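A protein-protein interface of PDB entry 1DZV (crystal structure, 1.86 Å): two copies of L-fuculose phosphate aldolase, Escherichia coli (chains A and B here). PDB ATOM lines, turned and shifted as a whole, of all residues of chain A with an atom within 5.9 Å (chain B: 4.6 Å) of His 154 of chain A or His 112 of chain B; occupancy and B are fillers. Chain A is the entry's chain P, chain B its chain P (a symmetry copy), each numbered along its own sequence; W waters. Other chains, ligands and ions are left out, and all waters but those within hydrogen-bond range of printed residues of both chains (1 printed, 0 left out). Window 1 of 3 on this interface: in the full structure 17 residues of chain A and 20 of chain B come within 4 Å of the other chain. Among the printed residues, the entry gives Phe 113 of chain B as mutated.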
ATOM      1  N   HIS A  94     -11.749   1.056 -11.472  1.00  0.00           N
ATOM      2  CA  HIS A  94     -12.639   1.229 -12.601  1.00  0.00           C
ATOM      3  C   HIS A  94     -11.830   0.949 -13.884  1.00  0.00           C
ATOM      4  O   HIS A  94     -11.866   1.721 -14.831  1.00  0.00           O
ATOM      5  CB  HIS A  94     -13.300   2.599 -12.622  1.00  0.00           C
ATOM      6  CG  HIS A  94     -14.058   3.043 -11.413  1.00  0.00           C
ATOM      7  ND1 HIS A  94     -14.576   4.314 -11.293  1.00  0.00           N
ATOM      8  CD2 HIS A  94     -14.414   2.409 -10.262  1.00  0.00           C
ATOM      9  CE1 HIS A  94     -15.186   4.450 -10.120  1.00  0.00           C
ATOM     10  NE2 HIS A  94     -15.100   3.288  -9.465  1.00  0.00           N
ATOM     11  N   THR A  99     -14.806  -2.549 -16.722  1.00  0.00           N
ATOM     12  CA  THR A  99     -15.953  -1.622 -16.651  1.00  0.00           C
ATOM     13  C   THR A  99     -16.796  -1.692 -17.911  1.00  0.00           C
ATOM     14  O   THR A  99     -18.043  -1.673 -17.806  1.00  0.00           O
ATOM     15  CB  THR A  99     -15.447  -0.193 -16.371  1.00  0.00           C
ATOM     16  OG1 THR A  99     -14.638  -0.205 -15.175  1.00  0.00           O
ATOM     17  CG2 THR A  99     -16.637   0.747 -16.170  1.00  0.00           C
ATOM     18  N   SER A 102     -18.878  -4.568 -17.539  1.00  0.00           N
ATOM     19  CA  SER A 102     -19.923  -4.310 -16.552  1.00  0.00           C
ATOM     20  C   SER A 102     -21.072  -3.481 -17.110  1.00  0.00           C
ATOM     21  O   SER A 102     -22.201  -3.605 -16.598  1.00  0.00           O
ATOM     22  CB  SER A 102     -19.355  -3.624 -15.311  1.00  0.00           C
ATOM     23  OG  SER A 102     -19.329  -2.221 -15.494  1.00  0.00           O
ATOM     24  N   ILE A 103     -20.804  -2.668 -18.119  1.00  0.00           N
ATOM     25  CA  ILE A 103     -21.862  -1.896 -18.771  1.00  0.00           C
ATOM     26  C   ILE A 103     -22.785  -2.796 -19.562  1.00  0.00           C
ATOM     27  O   ILE A 103     -24.014  -2.621 -19.600  1.00  0.00           O
ATOM     28  CB  ILE A 103     -21.208  -0.794 -19.623  1.00  0.00           C
ATOM     29  CG1 ILE A 103     -20.659   0.272 -18.677  1.00  0.00           C
ATOM     30  CG2 ILE A 103     -22.195  -0.167 -20.570  1.00  0.00           C
ATOM     31  CD1 ILE A 103     -19.720   1.269 -19.319  1.00  0.00           C
ATOM     32  N   CYS A 125     -21.083 -10.594 -12.542  1.00  0.00           N
ATOM     33  CA  CYS A 125     -21.326  -9.159 -12.642  1.00  0.00           C
ATOM     34  C   CYS A 125     -22.495  -8.854 -11.694  1.00  0.00           C
ATOM     35  O   CYS A 125     -23.599  -9.327 -11.960  1.00  0.00           O
ATOM     36  CB  CYS A 125     -21.680  -8.752 -14.070  1.00  0.00           C
ATOM     37  SG  CYS A 125     -21.917  -6.966 -14.227  1.00  0.00           S
ATOM     38  N   TYR A 128     -26.329  -3.274 -10.495  1.00  0.00           N
ATOM     39  CA  TYR A 128     -26.118  -1.900 -10.116  1.00  0.00           C
ATOM     40  C   TYR A 128     -26.826  -1.464  -8.833  1.00  0.00           C
ATOM     41  O   TYR A 128     -28.000  -1.764  -8.645  1.00  0.00           O
ATOM     42  CB  TYR A 128     -26.643  -0.981 -11.273  1.00  0.00           C
ATOM     43  CG  TYR A 128     -26.388   0.472 -10.881  1.00  0.00           C
ATOM     44  CD1 TYR A 128     -25.120   0.997 -10.975  1.00  0.00           C
ATOM     45  CD2 TYR A 128     -27.393   1.275 -10.373  1.00  0.00           C
ATOM     46  CE1 TYR A 128     -24.844   2.300 -10.593  1.00  0.00           C
ATOM     47  CE2 TYR A 128     -27.140   2.582 -10.001  1.00  0.00           C
ATOM     48  CZ  TYR A 128     -25.880   3.095 -10.115  1.00  0.00           C
ATOM     49  OH  TYR A 128     -25.584   4.374  -9.751  1.00  0.00           O
ATOM     50  N   LEU A 152     -18.914  -5.077 -11.233  1.00  0.00           N
ATOM     51  CA  LEU A 152     -20.042  -4.347 -10.623  1.00  0.00           C
ATOM     52  C   LEU A 152     -20.731  -3.590 -11.771  1.00  0.00           C
ATOM     53  O   LEU A 152     -20.060  -2.740 -12.363  1.00  0.00           O
ATOM     54  CB  LEU A 152     -19.506  -3.337  -9.614  1.00  0.00           C
ATOM     55  CG  LEU A 152     -18.941  -3.898  -8.291  1.00  0.00           C
ATOM     56  CD1 LEU A 152     -17.523  -4.396  -8.474  1.00  0.00           C
ATOM     57  CD2 LEU A 152     -18.887  -2.795  -7.248  1.00  0.00           C
ATOM     58  N   GLN A 153     -21.971  -3.923 -12.086  1.00  0.00           N
ATOM     59  CA  GLN A 153     -22.667  -3.295 -13.204  1.00  0.00           C
ATOM     60  C   GLN A 153     -22.597  -1.788 -13.251  1.00  0.00           C
ATOM     61  O   GLN A 153     -22.802  -1.109 -12.257  1.00  0.00           O
ATOM     62  CB  GLN A 153     -24.115  -3.805 -13.217  1.00  0.00           C
ATOM     63  CG  GLN A 153     -24.878  -3.246 -14.421  1.00  0.00           C
ATOM     64  CD  GLN A 153     -26.370  -3.543 -14.377  1.00  0.00           C
ATOM     65  OE1 GLN A 153     -27.057  -3.438 -15.405  1.00  0.00           O
ATOM     66  NE2 GLN A 153     -26.875  -3.990 -13.255  1.00  0.00           N
ATOM     67  N   HIS A 154     -22.236  -1.195 -14.386  1.00  0.00           N
ATOM     68  CA  HIS A 154     -22.062   0.221 -14.616  1.00  0.00           C
ATOM     69  C   HIS A 154     -21.059   0.853 -13.652  1.00  0.00           C
ATOM     70  O   HIS A 154     -21.206   2.018 -13.248  1.00  0.00           O
ATOM     71  CB  HIS A 154     -23.379   1.018 -14.498  1.00  0.00           C
ATOM     72  CG  HIS A 154     -24.328   0.766 -15.619  1.00  0.00           C
ATOM     73  ND1 HIS A 154     -24.141   1.248 -16.904  1.00  0.00           N
ATOM     74  CD2 HIS A 154     -25.496   0.070 -15.632  1.00  0.00           C
ATOM     75  CE1 HIS A 154     -25.157   0.836 -17.657  1.00  0.00           C
ATOM     76  NE2 HIS A 154     -25.992   0.115 -16.915  1.00  0.00           N
ATOM     77  N   HIS A 155     -19.989   0.116 -13.298  1.00  0.00           N
ATOM     78  CA  HIS A 155     -19.133   0.696 -12.251  1.00  0.00           C
ATOM     79  C   HIS A 155     -17.682   0.259 -12.378  1.00  0.00           C
ATOM     80  O   HIS A 155     -16.827   1.111 -12.631  1.00  0.00           O
ATOM     81  CB  HIS A 155     -19.760   0.248 -10.927  1.00  0.00           C
ATOM     82  CG  HIS A 155     -19.108   0.833  -9.716  1.00  0.00           C
ATOM     83  ND1 HIS A 155     -19.822   1.058  -8.571  1.00  0.00           N
ATOM     84  CD2 HIS A 155     -17.846   1.252  -9.464  1.00  0.00           C
ATOM     85  CE1 HIS A 155     -19.005   1.586  -7.666  1.00  0.00           C
ATOM     86  NE2 HIS A 155     -17.785   1.712  -8.169  1.00  0.00           N
ATOM     87  N   GLY A 156     -17.396  -1.026 -12.151  1.00  0.00           N
ATOM     88  CA  GLY A 156     -15.987  -1.430 -12.183  1.00  0.00           C
ATOM     89  C   GLY A 156     -15.749  -2.820 -11.628  1.00  0.00           C
ATOM     90  O   GLY A 156     -16.546  -3.731 -11.882  1.00  0.00           O
ATOM     91  N   ALA B 110     -25.406   8.355 -20.316  1.00  0.00           N
ATOM     92  CA  ALA B 110     -25.035   7.908 -18.976  1.00  0.00           C
ATOM     93  C   ALA B 110     -24.782   6.418 -18.866  1.00  0.00           C
ATOM     94  O   ALA B 110     -25.510   5.665 -18.197  1.00  0.00           O
ATOM     95  CB  ALA B 110     -26.113   8.331 -17.983  1.00  0.00           C
ATOM     96  N   ILE B 111     -23.673   5.971 -19.446  1.00  0.00           N
ATOM     97  CA  ILE B 111     -23.280   4.574 -19.430  1.00  0.00           C
ATOM     98  C   ILE B 111     -22.495   4.206 -18.172  1.00  0.00           C
ATOM     99  O   ILE B 111     -22.237   3.037 -17.891  1.00  0.00           O
ATOM    100  CB  ILE B 111     -22.412   4.260 -20.660  1.00  0.00           C
ATOM    101  CG1 ILE B 111     -21.191   5.183 -20.680  1.00  0.00           C
ATOM    102  CG2 ILE B 111     -23.272   4.436 -21.910  1.00  0.00           C
ATOM    103  CD1 ILE B 111     -20.125   4.772 -21.670  1.00  0.00           C
ATOM    104  N   HIS B 112     -22.146   5.197 -17.380  1.00  0.00           N
ATOM    105  CA  HIS B 112     -21.393   5.026 -16.144  1.00  0.00           C
ATOM    106  C   HIS B 112     -21.739   6.199 -15.231  1.00  0.00           C
ATOM    107  O   HIS B 112     -21.976   7.300 -15.774  1.00  0.00           O
ATOM    108  CB  HIS B 112     -19.889   5.065 -16.436  1.00  0.00           C
ATOM    109  CG  HIS B 112     -19.050   4.560 -15.297  1.00  0.00           C
ATOM    110  ND1 HIS B 112     -18.759   5.326 -14.196  1.00  0.00           N
ATOM    111  CD2 HIS B 112     -18.494   3.345 -15.069  1.00  0.00           C
ATOM    112  CE1 HIS B 112     -18.041   4.639 -13.334  1.00  0.00           C
ATOM    113  NE2 HIS B 112     -17.843   3.431 -13.846  1.00  0.00           N
ATOM    114  N   PHE B 113     -21.743   6.014 -13.919  1.00  0.00           N
ATOM    115  CA  PHE B 113     -22.140   7.124 -13.051  1.00  0.00           C
ATOM    116  C   PHE B 113     -21.139   8.254 -12.981  1.00  0.00           C
ATOM    117  O   PHE B 113     -21.545   9.382 -12.666  1.00  0.00           O
ATOM    118  CB  PHE B 113     -22.518   6.622 -11.658  1.00  0.00           C
ATOM    119  CG  PHE B 113     -21.328   6.098 -10.911  1.00  0.00           C
ATOM    120  CD1 PHE B 113     -20.554   6.934 -10.142  1.00  0.00           C
ATOM    121  CD2 PHE B 113     -21.023   4.748 -10.989  1.00  0.00           C
ATOM    122  CE1 PHE B 113     -19.451   6.438  -9.462  1.00  0.00           C
ATOM    123  CE2 PHE B 113     -19.927   4.243 -10.300  1.00  0.00           C
ATOM    124  CZ  PHE B 113     -19.148   5.098  -9.545  1.00  0.00           C
ATOM    125  N   MET B 114     -19.881   8.090 -13.384  1.00  0.00           N
ATOM    126  CA  MET B 114     -18.952   9.193 -13.403  1.00  0.00           C
ATOM    127  C   MET B 114     -19.283  10.252 -14.445  1.00  0.00           C
ATOM    128  O   MET B 114     -18.686  11.336 -14.395  1.00  0.00           O
ATOM    129  CB  MET B 114     -17.515   8.697 -13.595  1.00  0.00           C
ATOM    130  CG  MET B 114     -17.000   8.044 -12.313  1.00  0.00           C
ATOM    131  SD  MET B 114     -16.870   9.214 -10.944  1.00  0.00           S
ATOM    132  CE  MET B 114     -15.805  10.453 -11.670  1.00  0.00           C
ATOM    133  N   ILE B 115     -20.249  10.039 -15.321  1.00  0.00           N
ATOM    134  CA  ILE B 115     -20.660  11.082 -16.255  1.00  0.00           C
ATOM    135  C   ILE B 115     -21.149  12.317 -15.530  1.00  0.00           C
ATOM    136  O   ILE B 115     -21.000  13.434 -16.030  1.00  0.00           O
ATOM    137  CB  ILE B 115     -21.752  10.543 -17.203  1.00  0.00           C
ATOM    138  CG1 ILE B 115     -21.915  11.538 -18.355  1.00  0.00           C
ATOM    139  CG2 ILE B 115     -23.077  10.362 -16.521  1.00  0.00           C
ATOM    140  CD1 ILE B 115     -22.088  10.851 -19.684  1.00  0.00           C
ATOM    141  N   LEU B 177     -14.673   7.719 -20.331  1.00  0.00           N
ATOM    142  CA  LEU B 177     -16.072   7.502 -20.709  1.00  0.00           C
ATOM    143  C   LEU B 177     -16.236   7.305 -22.217  1.00  0.00           C
ATOM    144  O   LEU B 177     -16.988   6.458 -22.713  1.00  0.00           O
ATOM    145  CB  LEU B 177     -16.889   8.734 -20.283  1.00  0.00           C
ATOM    146  CG  LEU B 177     -17.205   8.870 -18.796  1.00  0.00           C
ATOM    147  CD1 LEU B 177     -17.808  10.231 -18.443  1.00  0.00           C
ATOM    148  CD2 LEU B 177     -18.125   7.732 -18.342  1.00  0.00           C
ATOM    149  N   LEU B 180     -15.082   3.848 -23.019  1.00  0.00           N
ATOM    150  CA  LEU B 180     -16.113   2.902 -22.599  1.00  0.00           C
ATOM    151  C   LEU B 180     -17.257   2.833 -23.623  1.00  0.00           C
ATOM    152  O   LEU B 180     -17.768   1.778 -23.978  1.00  0.00           O
ATOM    153  CB  LEU B 180     -16.710   3.265 -21.237  1.00  0.00           C
ATOM    154  CG  LEU B 180     -15.784   3.090 -20.035  1.00  0.00           C
ATOM    155  CD1 LEU B 180     -16.430   3.697 -18.799  1.00  0.00           C
ATOM    156  CD2 LEU B 180     -15.469   1.602 -19.819  1.00  0.00           C
ATOM    157  N   PRO B 192     -26.613   0.127 -22.946  1.00  0.00           N
ATOM    158  CA  PRO B 192     -27.398   0.285 -21.729  1.00  0.00           C
ATOM    159  C   PRO B 192     -27.048   1.568 -21.017  1.00  0.00           C
ATOM    160  O   PRO B 192     -25.865   1.872 -20.987  1.00  0.00           O
ATOM    161  CB  PRO B 192     -26.991  -0.919 -20.876  1.00  0.00           C
ATOM    162  CG  PRO B 192     -26.692  -1.954 -21.923  1.00  0.00           C
ATOM    163  CD  PRO B 192     -25.987  -1.202 -23.038  1.00  0.00           C
ATOM    164  N   VAL B 193     -27.986   2.304 -20.452  1.00  0.00           N
ATOM    165  CA  VAL B 193     -27.679   3.500 -19.696  1.00  0.00           C
ATOM    166  C   VAL B 193     -28.337   3.498 -18.314  1.00  0.00           C
ATOM    167  O   VAL B 193     -29.300   2.768 -18.102  1.00  0.00           O
ATOM    168  CB  VAL B 193     -28.139   4.808 -20.375  1.00  0.00           C
ATOM    169  CG1 VAL B 193     -27.303   5.067 -21.620  1.00  0.00           C
ATOM    170  CG2 VAL B 193     -29.635   4.785 -20.671  1.00  0.00           C
ATOM    171  N   LEU B 194     -27.839   4.339 -17.420  1.00  0.00           N
ATOM    172  CA  LEU B 194     -28.474   4.537 -16.120  1.00  0.00           C
ATOM    173  C   LEU B 194     -29.630   5.522 -16.333  1.00  0.00           C
ATOM    174  O   LEU B 194     -29.513   6.428 -17.153  1.00  0.00           O
ATOM    175  CB  LEU B 194     -27.478   5.119 -15.121  1.00  0.00           C
ATOM    176  CG  LEU B 194     -26.371   4.145 -14.680  1.00  0.00           C
ATOM    177  CD1 LEU B 194     -25.275   4.912 -13.950  1.00  0.00           C
ATOM    178  CD2 LEU B 194     -26.925   3.017 -13.831  1.00  0.00           C
HETATM  179  O   HOH W   1     -28.869  -0.062 -17.378  1.00  0.00           O
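Among the printed residues, pairs that only touch across the chains: Thr 99 of chain A with His 112 of chain B (3.4 Å), Thr 99 of chain A with Leu 180 of chain B (3.9 Å), Ile 103 of chain A with Ile 111 of chain B (3.3 Å), Ile 103 of chain A with Pro 192 of chain B (3.6 Å), Tyr 128 of chain A with Leu 194 of chain B (3.9 Å), His 154 of chain A with His 112 of chain B (3.5 Å), His 154 of chain A with Phe 113 of chain B (3.5 Å), His 154 of chain A with Pro 192 of chain B (3.6 Å), His 154 of chain A with Leu 194 of chain B (3.7 Å) and His 155 of chain A with Phe 113 of chain B (3.6 Å).
Water W1 lies within hydrogen-bond range of a ring nitrogen (NE2) of His 154 of chain A (2.9 Å) and the backbone carbonyl oxygen (O) of Val 193 of chain B (3.0 Å).
His 154 of chain A touches just these residues of chain B: Ile 111 (2.8 Å), His 112 (3.5 Å), Phe 113 (3.5 Å), Pro 192 (3.6 Å) and Leu 194 (3.7 Å). His 112 of chain B touches three residues of chain A. Printed residues of chain A within 4 Å of Phe 113 of chain B: His 154 (3.5 Å) and His 155 (3.6 Å). Of the printed residues of chain A, Leu 194 of chain B touches Tyr 128 and His 154. Of the printed residues of chain A, Pro 192 of chain B touches Ile 103 and His 154. Of the printed residues of chain A, Leu 180 of chain B touches Thr 99. Printed residues of chain A within 4 Å of Ile 111 of chain B: Ile 103 (3.3 Å) and His 154 (2.8 Å). Leu 177 of chain B touches none of the printed residues of chain A. Gln 153 of chain A touches none of the printed residues of chain B. The nearest residue of chain B that does not touch His 154 of chain A is Val 193 of chain B (4.2 Å). The nearest residue of chain A that does not touch His 112 of chain B is His 94 of chain A (4.03 Å). The nearest printed residue of chain A that does not touch Ile 111 of chain B is His 155 of chain A (5.9 Å).
The backbone carbonyl oxygen of His 155 of chain A is in hydrogen-bond range of a ring nitrogen (NE2) of His 112 of chain B, at 2.8 Å. A ring nitrogen (ND1) of His 154 of chain A lies within hydrogen-bond range of the backbone carbonyl oxygen (O) of Ile 111 of chain B (2.8 Å).
Of the 11 printed residues of chain A, 5 touch a printed residue of chain B. Of the 11 printed residues of chain B, 6 touch a printed residue of chain A. Among the printed residues, 12 pairs touch across the chains. Among the printed residues, no Asp or Glu carboxylate lies within 4 Å of a Lys or Arg side-chain nitrogen of the other chain.
O of Ser 102 of chain A lies within hydrogen-bond range of N of His 154 of chain A (3.3 Å). O of His 94 of chain A sits close to OG1 of Thr 99 of chain A, at 3.4 Å. The side-chain amide nitrogen (NE2) of Gln 153 of chain A sits close to the backbone NH (N) of Tyr 128 of chain A (2.9 Å). N of Met 114 of chain B is in hydrogen-bond range of ND1 of His 112 of chain B (3.1 Å). N of His 155 of chain A sits at hydrogen-bond distance from OG of Ser 102 of chain A, 3.3 Å away. OG of Ser 102 of chain A sits at hydrogen-bond distance from O of Thr 99 of chain A.
No position is printed for both chains. Of the 12 pairs that touch across the chains among the printed residues, none has its exchanged pair printed and touching as well.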
